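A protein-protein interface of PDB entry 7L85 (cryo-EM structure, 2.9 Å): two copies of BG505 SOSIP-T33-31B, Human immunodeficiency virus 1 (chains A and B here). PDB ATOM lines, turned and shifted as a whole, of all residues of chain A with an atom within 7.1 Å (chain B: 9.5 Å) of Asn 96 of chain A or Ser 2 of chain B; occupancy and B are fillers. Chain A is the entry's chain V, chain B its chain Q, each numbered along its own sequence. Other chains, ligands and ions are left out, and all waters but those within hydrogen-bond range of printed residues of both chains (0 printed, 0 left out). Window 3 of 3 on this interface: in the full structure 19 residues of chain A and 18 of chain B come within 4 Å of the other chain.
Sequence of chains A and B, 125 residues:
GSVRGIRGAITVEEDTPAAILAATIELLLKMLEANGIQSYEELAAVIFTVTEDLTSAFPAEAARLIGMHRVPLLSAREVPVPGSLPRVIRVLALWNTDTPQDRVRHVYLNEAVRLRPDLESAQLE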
ATOM      1  N   GLY A   1     -29.281 -31.391  14.002  1.00  0.00           N
ATOM      2  CA  GLY A   1     -30.039 -30.192  13.682  1.00  0.00           C
ATOM      3  C   GLY A   1     -29.717 -29.692  12.289  1.00  0.00           C
ATOM      4  O   GLY A   1     -28.758 -30.123  11.645  1.00  0.00           O
ATOM      5  N   SER A   2     -30.505 -28.744  11.828  1.00  0.00           N
ATOM      6  CA  SER A   2     -30.332 -28.146  10.530  1.00  0.00           C
ATOM      7  C   SER A   2     -30.587 -26.673  10.635  1.00  0.00           C
ATOM      8  O   SER A   2     -30.547 -26.118  11.722  1.00  0.00           O
ATOM      9  CB  SER A   2     -31.281 -28.757   9.562  1.00  0.00           C
ATOM     10  OG  SER A   2     -30.949 -28.364   8.294  1.00  0.00           O
ATOM     11  N   VAL A   3     -30.759 -26.008   9.517  1.00  0.00           N
ATOM     12  CA  VAL A   3     -30.995 -24.576   9.579  1.00  0.00           C
ATOM     13  C   VAL A   3     -32.250 -24.172   8.874  1.00  0.00           C
ATOM     14  O   VAL A   3     -32.500 -24.548   7.729  1.00  0.00           O
ATOM     15  CB  VAL A   3     -29.823 -23.781   9.021  1.00  0.00           C
ATOM     16  CG1 VAL A   3     -30.104 -22.287   9.078  1.00  0.00           C
ATOM     17  CG2 VAL A   3     -28.652 -24.068   9.817  1.00  0.00           C
ATOM     18  N   ARG A   4     -33.065 -23.406   9.558  1.00  0.00           N
ATOM     19  CA  ARG A   4     -34.269 -22.918   8.949  1.00  0.00           C
ATOM     20  C   ARG A   4     -34.321 -21.434   9.066  1.00  0.00           C
ATOM     21  O   ARG A   4     -34.078 -20.892  10.139  1.00  0.00           O
ATOM     22  CB  ARG A   4     -35.488 -23.465   9.645  1.00  0.00           C
ATOM     23  CG  ARG A   4     -35.592 -24.948   9.712  1.00  0.00           C
ATOM     24  CD  ARG A   4     -35.827 -25.518   8.428  1.00  0.00           C
ATOM     25  NE  ARG A   4     -35.927 -26.924   8.488  1.00  0.00           N
ATOM     26  CZ  ARG A   4     -35.836 -27.719   7.418  1.00  0.00           C
ATOM     27  NH1 ARG A   4     -35.652 -27.187   6.220  1.00  0.00           N
ATOM     28  NH2 ARG A   4     -35.933 -29.025   7.558  1.00  0.00           N
ATOM     29  N   GLU A  41     -29.214 -18.459  21.731  1.00  0.00           N
ATOM     30  CA  GLU A  41     -28.147 -19.384  21.442  1.00  0.00           C
ATOM     31  C   GLU A  41     -28.458 -20.206  20.220  1.00  0.00           C
ATOM     32  O   GLU A  41     -27.576 -20.821  19.626  1.00  0.00           O
ATOM     33  CB  GLU A  41     -27.907 -20.288  22.620  1.00  0.00           C
ATOM     34  CG  GLU A  41     -27.323 -19.579  23.792  1.00  0.00           C
ATOM     35  CD  GLU A  41     -27.205 -20.454  24.978  1.00  0.00           C
ATOM     36  OE1 GLU A  41     -27.796 -21.507  24.963  1.00  0.00           O
ATOM     37  OE2 GLU A  41     -26.527 -20.086  25.904  1.00  0.00           O
ATOM     38  N   GLU A  42     -29.727 -20.269  19.855  1.00  0.00           N
ATOM     39  CA  GLU A  42     -30.118 -21.058  18.720  1.00  0.00           C
ATOM     40  C   GLU A  42     -30.021 -20.263  17.425  1.00  0.00           C
ATOM     41  O   GLU A  42     -30.245 -20.809  16.350  1.00  0.00           O
ATOM     42  CB  GLU A  42     -31.545 -21.549  18.911  1.00  0.00           C
ATOM     43  CG  GLU A  42     -31.738 -22.453  20.107  1.00  0.00           C
ATOM     44  CD  GLU A  42     -33.180 -22.930  20.301  1.00  0.00           C
ATOM     45  OE1 GLU A  42     -34.025 -22.678  19.466  1.00  0.00           O
ATOM     46  OE2 GLU A  42     -33.429 -23.548  21.309  1.00  0.00           O
ATOM     47  N   LEU A  43     -29.728 -18.975  17.493  1.00  0.00           N
ATOM     48  CA  LEU A  43     -29.698 -18.192  16.279  1.00  0.00           C
ATOM     49  C   LEU A  43     -28.308 -18.073  15.728  1.00  0.00           C
ATOM     50  O   LEU A  43     -27.385 -17.631  16.408  1.00  0.00           O
ATOM     51  CB  LEU A  43     -30.258 -16.820  16.559  1.00  0.00           C
ATOM     52  CG  LEU A  43     -31.663 -16.793  17.099  1.00  0.00           C
ATOM     53  CD1 LEU A  43     -31.972 -15.405  17.458  1.00  0.00           C
ATOM     54  CD2 LEU A  43     -32.658 -17.324  16.070  1.00  0.00           C
ATOM     55  N   ALA A  44     -28.147 -18.509  14.493  1.00  0.00           N
ATOM     56  CA  ALA A  44     -26.870 -18.457  13.838  1.00  0.00           C
ATOM     57  C   ALA A  44     -26.553 -17.044  13.470  1.00  0.00           C
ATOM     58  O   ALA A  44     -25.406 -16.612  13.554  1.00  0.00           O
ATOM     59  CB  ALA A  44     -26.873 -19.306  12.584  1.00  0.00           C
ATOM     60  N   ALA A  45     -27.575 -16.348  12.998  1.00  0.00           N
ATOM     61  CA  ALA A  45     -27.433 -14.959  12.565  1.00  0.00           C
ATOM     62  C   ALA A  45     -28.769 -14.307  12.326  1.00  0.00           C
ATOM     63  O   ALA A  45     -29.754 -14.997  12.064  1.00  0.00           O
ATOM     64  CB  ALA A  45     -26.619 -14.877  11.302  1.00  0.00           C
ATOM     65  N   LEU A  94     -31.646 -16.865  11.006  1.00  0.00           N
ATOM     66  CA  LEU A  94     -31.241 -18.224  10.726  1.00  0.00           C
ATOM     67  C   LEU A  94     -31.162 -18.984  12.011  1.00  0.00           C
ATOM     68  O   LEU A  94     -30.368 -18.658  12.899  1.00  0.00           O
ATOM     69  CB  LEU A  94     -29.929 -18.227   9.980  1.00  0.00           C
ATOM     70  CG  LEU A  94     -29.917 -17.474   8.661  1.00  0.00           C
ATOM     71  CD1 LEU A  94     -28.535 -17.508   8.120  1.00  0.00           C
ATOM     72  CD2 LEU A  94     -30.908 -18.093   7.664  1.00  0.00           C
ATOM     73  N   TRP A  95     -32.066 -19.939  12.130  1.00  0.00           N
ATOM     74  CA  TRP A  95     -32.312 -20.726  13.315  1.00  0.00           C
ATOM     75  C   TRP A  95     -31.799 -22.156  13.276  1.00  0.00           C
ATOM     76  O   TRP A  95     -32.174 -22.957  12.412  1.00  0.00           O
ATOM     77  CB  TRP A  95     -33.801 -20.698  13.528  1.00  0.00           C
ATOM     78  CG  TRP A  95     -34.294 -21.308  14.703  1.00  0.00           C
ATOM     79  CD1 TRP A  95     -33.692 -21.446  15.870  1.00  0.00           C
ATOM     80  CD2 TRP A  95     -35.570 -21.864  14.853  1.00  0.00           C
ATOM     81  NE1 TRP A  95     -34.501 -22.051  16.728  1.00  0.00           N
ATOM     82  CE2 TRP A  95     -35.656 -22.312  16.121  1.00  0.00           C
ATOM     83  CE3 TRP A  95     -36.642 -22.010  14.013  1.00  0.00           C
ATOM     84  CZ2 TRP A  95     -36.755 -22.898  16.589  1.00  0.00           C
ATOM     85  CZ3 TRP A  95     -37.753 -22.600  14.483  1.00  0.00           C
ATOM     86  CH2 TRP A  95     -37.807 -23.036  15.737  1.00  0.00           C
ATOM     87  N   ASN A  96     -30.937 -22.504  14.211  1.00  0.00           N
ATOM     88  CA  ASN A  96     -30.358 -23.833  14.246  1.00  0.00           C
ATOM     89  C   ASN A  96     -31.246 -24.826  14.946  1.00  0.00           C
ATOM     90  O   ASN A  96     -31.011 -25.206  16.091  1.00  0.00           O
ATOM     91  CB  ASN A  96     -29.040 -23.809  14.939  1.00  0.00           C
ATOM     92  CG  ASN A  96     -28.027 -23.135  14.193  1.00  0.00           C
ATOM     93  OD1 ASN A  96     -27.920 -23.275  12.988  1.00  0.00           O
ATOM     94  ND2 ASN A  96     -27.225 -22.417  14.874  1.00  0.00           N
ATOM     95  N   THR A  97     -32.255 -25.250  14.239  1.00  0.00           N
ATOM     96  CA  THR A  97     -33.275 -26.144  14.746  1.00  0.00           C
ATOM     97  C   THR A  97     -33.454 -27.426  13.997  1.00  0.00           C
ATOM     98  O   THR A  97     -32.857 -27.649  12.954  1.00  0.00           O
ATOM     99  CB  THR A  97     -34.603 -25.451  14.723  1.00  0.00           C
ATOM    100  OG1 THR A  97     -35.569 -26.275  15.371  1.00  0.00           O
ATOM    101  CG2 THR A  97     -35.011 -25.155  13.291  1.00  0.00           C
ATOM    102  N   ASP A  98     -34.291 -28.296  14.535  1.00  0.00           N
ATOM    103  CA  ASP A  98     -34.672 -29.527  13.886  1.00  0.00           C
ATOM    104  C   ASP A  98     -36.128 -29.486  13.442  1.00  0.00           C
ATOM    105  O   ASP A  98     -36.684 -30.481  12.978  1.00  0.00           O
ATOM    106  CB  ASP A  98     -34.402 -30.674  14.828  1.00  0.00           C
ATOM    107  CG  ASP A  98     -35.116 -30.469  16.111  1.00  0.00           C
ATOM    108  OD1 ASP A  98     -35.529 -29.339  16.347  1.00  0.00           O
ATOM    109  OD2 ASP A  98     -35.242 -31.391  16.871  1.00  0.00           O
ATOM    110  N   THR A  99     -36.700 -28.307  13.519  1.00  0.00           N
ATOM    111  CA  THR A  99     -38.053 -28.028  13.115  1.00  0.00           C
ATOM    112  C   THR A  99     -38.136 -28.178  11.595  1.00  0.00           C
ATOM    113  O   THR A  99     -37.234 -27.701  10.907  1.00  0.00           O
ATOM    114  CB  THR A  99     -38.437 -26.602  13.528  1.00  0.00           C
ATOM    115  OG1 THR A  99     -38.294 -26.466  14.931  1.00  0.00           O
ATOM    116  CG2 THR A  99     -39.831 -26.297  13.178  1.00  0.00           C
ATOM    117  N   GLY B   1     -22.844 -30.910  13.801  1.00  0.00           N
ATOM    118  CA  GLY B   1     -22.455 -29.511  13.726  1.00  0.00           C
ATOM    119  C   GLY B   1     -23.662 -28.612  13.553  1.00  0.00           C
ATOM    120  O   GLY B   1     -24.775 -29.060  13.269  1.00  0.00           O
ATOM    121  N   SER B   2     -23.437 -27.322  13.690  1.00  0.00           N
ATOM    122  CA  SER B   2     -24.467 -26.329  13.543  1.00  0.00           C
ATOM    123  C   SER B   2     -23.907 -25.147  12.812  1.00  0.00           C
ATOM    124  O   SER B   2     -22.883 -25.263  12.154  1.00  0.00           O
ATOM    125  CB  SER B   2     -24.958 -25.910  14.882  1.00  0.00           C
ATOM    126  OG  SER B   2     -26.091 -25.156  14.734  1.00  0.00           O
ATOM    127  N   VAL B   3     -24.599 -24.036  12.835  1.00  0.00           N
ATOM    128  CA  VAL B   3     -24.092 -22.876  12.124  1.00  0.00           C
ATOM    129  C   VAL B   3     -23.971 -21.672  13.007  1.00  0.00           C
ATOM    130  O   VAL B   3     -24.897 -21.302  13.726  1.00  0.00           O
ATOM    131  CB  VAL B   3     -24.947 -22.528  10.915  1.00  0.00           C
ATOM    132  CG1 VAL B   3     -24.408 -21.297  10.203  1.00  0.00           C
ATOM    133  CG2 VAL B   3     -24.925 -23.647  10.001  1.00  0.00           C
ATOM    134  N   ARG B   4     -22.815 -21.055  12.969  1.00  0.00           N
ATOM    135  CA  ARG B   4     -22.620 -19.857  13.736  1.00  0.00           C
ATOM    136  C   ARG B   4     -22.144 -18.766  12.842  1.00  0.00           C
ATOM    137  O   ARG B   4     -21.234 -18.974  12.045  1.00  0.00           O
ATOM    138  CB  ARG B   4     -21.567 -20.061  14.793  1.00  0.00           C
ATOM    139  CG  ARG B   4     -21.810 -21.171  15.755  1.00  0.00           C
ATOM    140  CD  ARG B   4     -22.908 -20.887  16.619  1.00  0.00           C
ATOM    141  NE  ARG B   4     -23.141 -21.936  17.532  1.00  0.00           N
ATOM    142  CZ  ARG B   4     -24.269 -22.071  18.232  1.00  0.00           C
ATOM    143  NH1 ARG B   4     -25.240 -21.180  18.091  1.00  0.00           N
ATOM    144  NH2 ARG B   4     -24.415 -23.085  19.062  1.00  0.00           N
ATOM    145  N   GLY B   5     -22.719 -17.591  12.958  1.00  0.00           N
ATOM    146  CA  GLY B   5     -22.193 -16.519  12.166  1.00  0.00           C
ATOM    147  C   GLY B   5     -20.967 -15.929  12.835  1.00  0.00           C
ATOM    148  O   GLY B   5     -20.865 -15.924  14.060  1.00  0.00           O
ATOM    149  N   GLU B  42     -15.082 -25.065   5.817  1.00  0.00           N
ATOM    150  CA  GLU B  42     -16.029 -24.948   6.893  1.00  0.00           C
ATOM    151  C   GLU B  42     -16.974 -23.772   6.683  1.00  0.00           C
ATOM    152  O   GLU B  42     -17.894 -23.576   7.468  1.00  0.00           O
ATOM    153  CB  GLU B  42     -15.284 -24.775   8.208  1.00  0.00           C
ATOM    154  CG  GLU B  42     -14.402 -25.943   8.582  1.00  0.00           C
ATOM    155  CD  GLU B  42     -13.642 -25.756   9.899  1.00  0.00           C
ATOM    156  OE1 GLU B  42     -13.866 -24.789  10.601  1.00  0.00           O
ATOM    157  OE2 GLU B  42     -12.823 -26.592  10.192  1.00  0.00           O
ATOM    158  N   LEU B  43     -16.755 -22.959   5.663  1.00  0.00           N
ATOM    159  CA  LEU B  43     -17.601 -21.801   5.491  1.00  0.00           C
ATOM    160  C   LEU B  43     -18.717 -22.068   4.523  1.00  0.00           C
ATOM    161  O   LEU B  43     -18.497 -22.467   3.382  1.00  0.00           O
ATOM    162  CB  LEU B  43     -16.766 -20.644   5.002  1.00  0.00           C
ATOM    163  CG  LEU B  43     -15.616 -20.256   5.890  1.00  0.00           C
ATOM    164  CD1 LEU B  43     -14.835 -19.235   5.183  1.00  0.00           C
ATOM    165  CD2 LEU B  43     -16.116 -19.724   7.233  1.00  0.00           C
ATOM    166  N   ALA B  44     -19.935 -21.882   4.998  1.00  0.00           N
ATOM    167  CA  ALA B  44     -21.098 -22.101   4.184  1.00  0.00           C
ATOM    168  C   ALA B  44     -21.227 -20.995   3.188  1.00  0.00           C
ATOM    169  O   ALA B  44     -21.619 -21.219   2.045  1.00  0.00           O
ATOM    170  CB  ALA B  44     -22.350 -22.146   5.037  1.00  0.00           C
ATOM    171  N   LEU B  94     -20.748 -17.417   7.547  1.00  0.00           N
ATOM    172  CA  LEU B  94     -21.505 -18.495   8.145  1.00  0.00           C
ATOM    173  C   LEU B  94     -20.647 -19.717   8.204  1.00  0.00           C
ATOM    174  O   LEU B  94     -20.215 -20.247   7.175  1.00  0.00           O
ATOM    175  CB  LEU B  94     -22.774 -18.727   7.364  1.00  0.00           C
ATOM    176  CG  LEU B  94     -23.707 -17.533   7.250  1.00  0.00           C
ATOM    177  CD1 LEU B  94     -24.849 -17.919   6.380  1.00  0.00           C
ATOM    178  CD2 LEU B  94     -24.203 -17.086   8.633  1.00  0.00           C
ATOM    179  N   TRP B  95     -20.331 -20.095   9.429  1.00  0.00           N
ATOM    180  CA  TRP B  95     -19.401 -21.145   9.775  1.00  0.00           C
ATOM    181  C   TRP B  95     -20.026 -22.440  10.270  1.00  0.00           C
ATOM    182  O   TRP B  95     -20.755 -22.471  11.268  1.00  0.00           O
ATOM    183  CB  TRP B  95     -18.485 -20.564  10.815  1.00  0.00           C
ATOM    184  CG  TRP B  95     -17.402 -21.364  11.241  1.00  0.00           C
ATOM    185  CD1 TRP B  95     -16.753 -22.291  10.563  1.00  0.00           C
ATOM    186  CD2 TRP B  95     -16.782 -21.289  12.495  1.00  0.00           C
ATOM    187  NE1 TRP B  95     -15.780 -22.799  11.306  1.00  0.00           N
ATOM    188  CE2 TRP B  95     -15.784 -22.194  12.491  1.00  0.00           C
ATOM    189  CE3 TRP B  95     -16.994 -20.521  13.608  1.00  0.00           C
ATOM    190  CZ2 TRP B  95     -14.990 -22.371  13.545  1.00  0.00           C
ATOM    191  CZ3 TRP B  95     -16.194 -20.698  14.672  1.00  0.00           C
ATOM    192  CH2 TRP B  95     -15.220 -21.601  14.642  1.00  0.00           C
ATOM    193  N   ASN B  96     -19.748 -23.533   9.587  1.00  0.00           N
ATOM    194  CA  ASN B  96     -20.319 -24.816   9.951  1.00  0.00           C
ATOM    195  C   ASN B  96     -19.530 -25.506  11.033  1.00  0.00           C
ATOM    196  O   ASN B  96     -18.778 -26.444  10.781  1.00  0.00           O
ATOM    197  CB  ASN B  96     -20.380 -25.716   8.767  1.00  0.00           C
ATOM    198  CG  ASN B  96     -21.343 -25.300   7.798  1.00  0.00           C
ATOM    199  OD1 ASN B  96     -22.438 -24.882   8.124  1.00  0.00           O
ATOM    200  ND2 ASN B  96     -20.995 -25.438   6.580  1.00  0.00           N
ATOM    201  N   THR B  97     -19.729 -25.042  12.235  1.00  0.00           N
ATOM    202  CA  THR B  97     -19.015 -25.505  13.404  1.00  0.00           C
ATOM    203  C   THR B  97     -19.858 -26.043  14.517  1.00  0.00           C
ATOM    204  O   THR B  97     -21.079 -25.981  14.484  1.00  0.00           O
ATOM    205  CB  THR B  97     -18.217 -24.376  13.982  1.00  0.00           C
ATOM    206  OG1 THR B  97     -17.394 -24.880  15.032  1.00  0.00           O
ATOM    207  CG2 THR B  97     -19.146 -23.289  14.490  1.00  0.00           C
ATOM    208  N   ASP B  98     -19.202 -26.584  15.528  1.00  0.00           N
ATOM    209  CA  ASP B  98     -19.851 -27.039  16.733  1.00  0.00           C
ATOM    210  C   ASP B  98     -19.498 -26.148  17.916  1.00  0.00           C
ATOM    211  O   ASP B  98     -19.849 -26.432  19.061  1.00  0.00           O
ATOM    212  CB  ASP B  98     -19.465 -28.477  16.977  1.00  0.00           C
ATOM    213  CG  ASP B  98     -17.992 -28.613  17.046  1.00  0.00           C
ATOM    214  OD1 ASP B  98     -17.321 -27.685  16.605  1.00  0.00           O
ATOM    215  OD2 ASP B  98     -17.511 -29.619  17.496  1.00  0.00           O
ATOM    216  N   THR B  99     -18.872 -25.034  17.608  1.00  0.00           N
ATOM    217  CA  THR B  99     -18.480 -24.028  18.558  1.00  0.00           C
ATOM    218  C   THR B  99     -19.748 -23.383  19.117  1.00  0.00           C
ATOM    219  O   THR B  99     -20.656 -23.094  18.336  1.00  0.00           O
ATOM    220  CB  THR B  99     -17.607 -22.972  17.868  1.00  0.00           C
ATOM    221  OG1 THR B  99     -16.470 -23.600  17.305  1.00  0.00           O
ATOM    222  CG2 THR B  99     -17.144 -21.953  18.821  1.00  0.00           C
ATOM    223  N   PRO B 100     -19.884 -23.210  20.436  1.00  0.00           N
ATOM    224  CA  PRO B 100     -20.960 -22.529  21.115  1.00  0.00           C
ATOM    225  C   PRO B 100     -21.024 -21.100  20.669  1.00  0.00           C
ATOM    226  O   PRO B 100     -20.018 -20.533  20.280  1.00  0.00           O
ATOM    227  CB  PRO B 100     -20.565 -22.629  22.566  1.00  0.00           C
ATOM    228  CG  PRO B 100     -19.691 -23.809  22.635  1.00  0.00           C
ATOM    229  CD  PRO B 100     -18.960 -23.848  21.345  1.00  0.00           C
ATOM    230  N   GLN B 101     -22.182 -20.487  20.752  1.00  0.00           N
ATOM    231  CA  GLN B 101     -22.318 -19.121  20.295  1.00  0.00           C
ATOM    232  C   GLN B 101     -21.384 -18.177  21.005  1.00  0.00           C
ATOM    233  O   GLN B 101     -20.845 -17.251  20.407  1.00  0.00           O
ATOM    234  CB  GLN B 101     -23.739 -18.635  20.512  1.00  0.00           C
ATOM    235  CG  GLN B 101     -24.037 -17.285  19.949  1.00  0.00           C
ATOM    236  CD  GLN B 101     -25.422 -16.921  20.218  1.00  0.00           C
ATOM    237  OE1 GLN B 101     -25.753 -16.562  21.351  1.00  0.00           O
ATOM    238  NE2 GLN B 101     -26.273 -17.056  19.228  1.00  0.00           N
ATOM    239  N   VAL B 104     -17.509 -17.858  19.842  1.00  0.00           N
ATOM    240  CA  VAL B 104     -17.144 -17.386  18.528  1.00  0.00           C
ATOM    241  C   VAL B 104     -16.632 -15.987  18.683  1.00  0.00           C
ATOM    242  O   VAL B 104     -17.265 -15.163  19.331  1.00  0.00           O
ATOM    243  CB  VAL B 104     -18.327 -17.435  17.573  1.00  0.00           C
ATOM    244  CG1 VAL B 104     -17.941 -16.873  16.220  1.00  0.00           C
ATOM    245  CG2 VAL B 104     -18.772 -18.858  17.438  1.00  0.00           C
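The side-chain hydroxyl (OG) of Ser 2 of chain B lies close to the side-chain amide nitrogen (ND2) of Asn 96 of chain A (3.0 Å). The backbone carbonyl oxygen (O) of Val 3 of chain B sits at hydrogen-bond distance from the side-chain amide nitrogen (ND2) of Asn 96 of chain A (2.8 Å). The guanidinium group (NH1) of Arg 4 of chain B lies within hydrogen-bond range of the backbone carbonyl oxygen (O) of Glu 41 of chain A. The backbone carbonyl oxygen (O) of Ala 44 of chain A lies within hydrogen-bond range of the backbone NH (N) of Gly 5 of chain B (2.9 Å). The side-chain amide nitrogen of Gln 101 of chain B lies within hydrogen-bond range of the backbone carbonyl oxygen of Leu 43 of chain A, 3.1 Å away.
The backbone NH (N) of Ser 2 of chain B is in hydrogen-bond range of the backbone carbonyl oxygen (O) of Thr 97 of chain B (2.8 Å). The backbone carbonyl oxygen (O) of Arg 4 of chain B is in hydrogen-bond range of the backbone NH (N) of Trp 95 of chain B (3.0 Å). The guanidinium group (NE) of Arg 4 of chain B sits at hydrogen-bond distance from the backbone carbonyl oxygen (O) of Thr 99 of chain B (2.9 Å). N of Asn 96 of chain A lies within hydrogen-bond range of O of Glu 42 of chain A. N of Ala 44 of chain A is in hydrogen-bond range of O of Leu 94 of chain A (2.7 Å).
Val 3 of chain A touches Val 3 of chain B (CG2 to CG2, 3.8 Å). CA of Glu 41 of chain A touches OE1 of Gln 101 of chain B (3.7 Å). CB of Ala 44 of chain A touches O of Val 3 of chain B, 3.0 Å away. Ala 44 of chain A touches Arg 4 of chain B. Asn 96 of chain A touches Arg 4 of chain B.
Of chain B, only Ser 2 (2.9 Å), Val 3 (2.8 Å) and Arg 4 (3.98 Å) come within 4 Å of Asn 96 of chain A. Ser 2 of chain B touches just one residue of chain A: Asn 96. Of the printed residues of chain A, Gln 101 of chain B touches Glu 41 and Leu 43. Of the printed residues of chain B, Leu 43 of chain A touches Gln 101. Of the printed residues of chain B, Ala 44 of chain A touches Val 3, Arg 4 and Gly 5. Of the printed residues of chain A, Arg 4 of chain B touches Glu 41 (2.8 Å), Ala 44 (3.97 Å) and Asn 96 (3.98 Å). Of the printed residues of chain B, Glu 41 of chain A touches Arg 4 and Gln 101. The nearest residue of chain B that does not touch Asn 96 of chain A is Gly 1 of chain B (6.6 Å). The nearest printed residue of chain B that does not touch Leu 43 of chain A is Arg 4 of chain B (4.5 Å).
Hydrophobic or aromatic side chains of chain B within 4 Å of the printed part of chain A: Val 3. Among the printed residues, 10 pairs touch across the chains. Among the printed residues, no Asp or Glu carboxylate lies within 4 Å of a Lys or Arg side-chain nitrogen of the other chain.
Val 3 of chain B touches its own counterpart, Val 3 of chain A. Ala 44 of chain A touches Val 3 of chain B, but with the chains exchanged Val 3 of chain A does not touch Ala 44 of chain B (8.1 Å). Asn 96 of chain A touches Val 3 of chain B, but with the chains exchanged Val 3 of chain A does not touch Asn 96 of chain B (6.5 Å). Asn 96 of chain A touches Arg 4 of chain B, but with the chains exchanged Arg 4 of chain A does not touch Asn 96 of chain B (10.8 Å). Of the 10 pairs that touch across the chains among the printed residues, 1 has its exchanged pair printed and touching as well.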
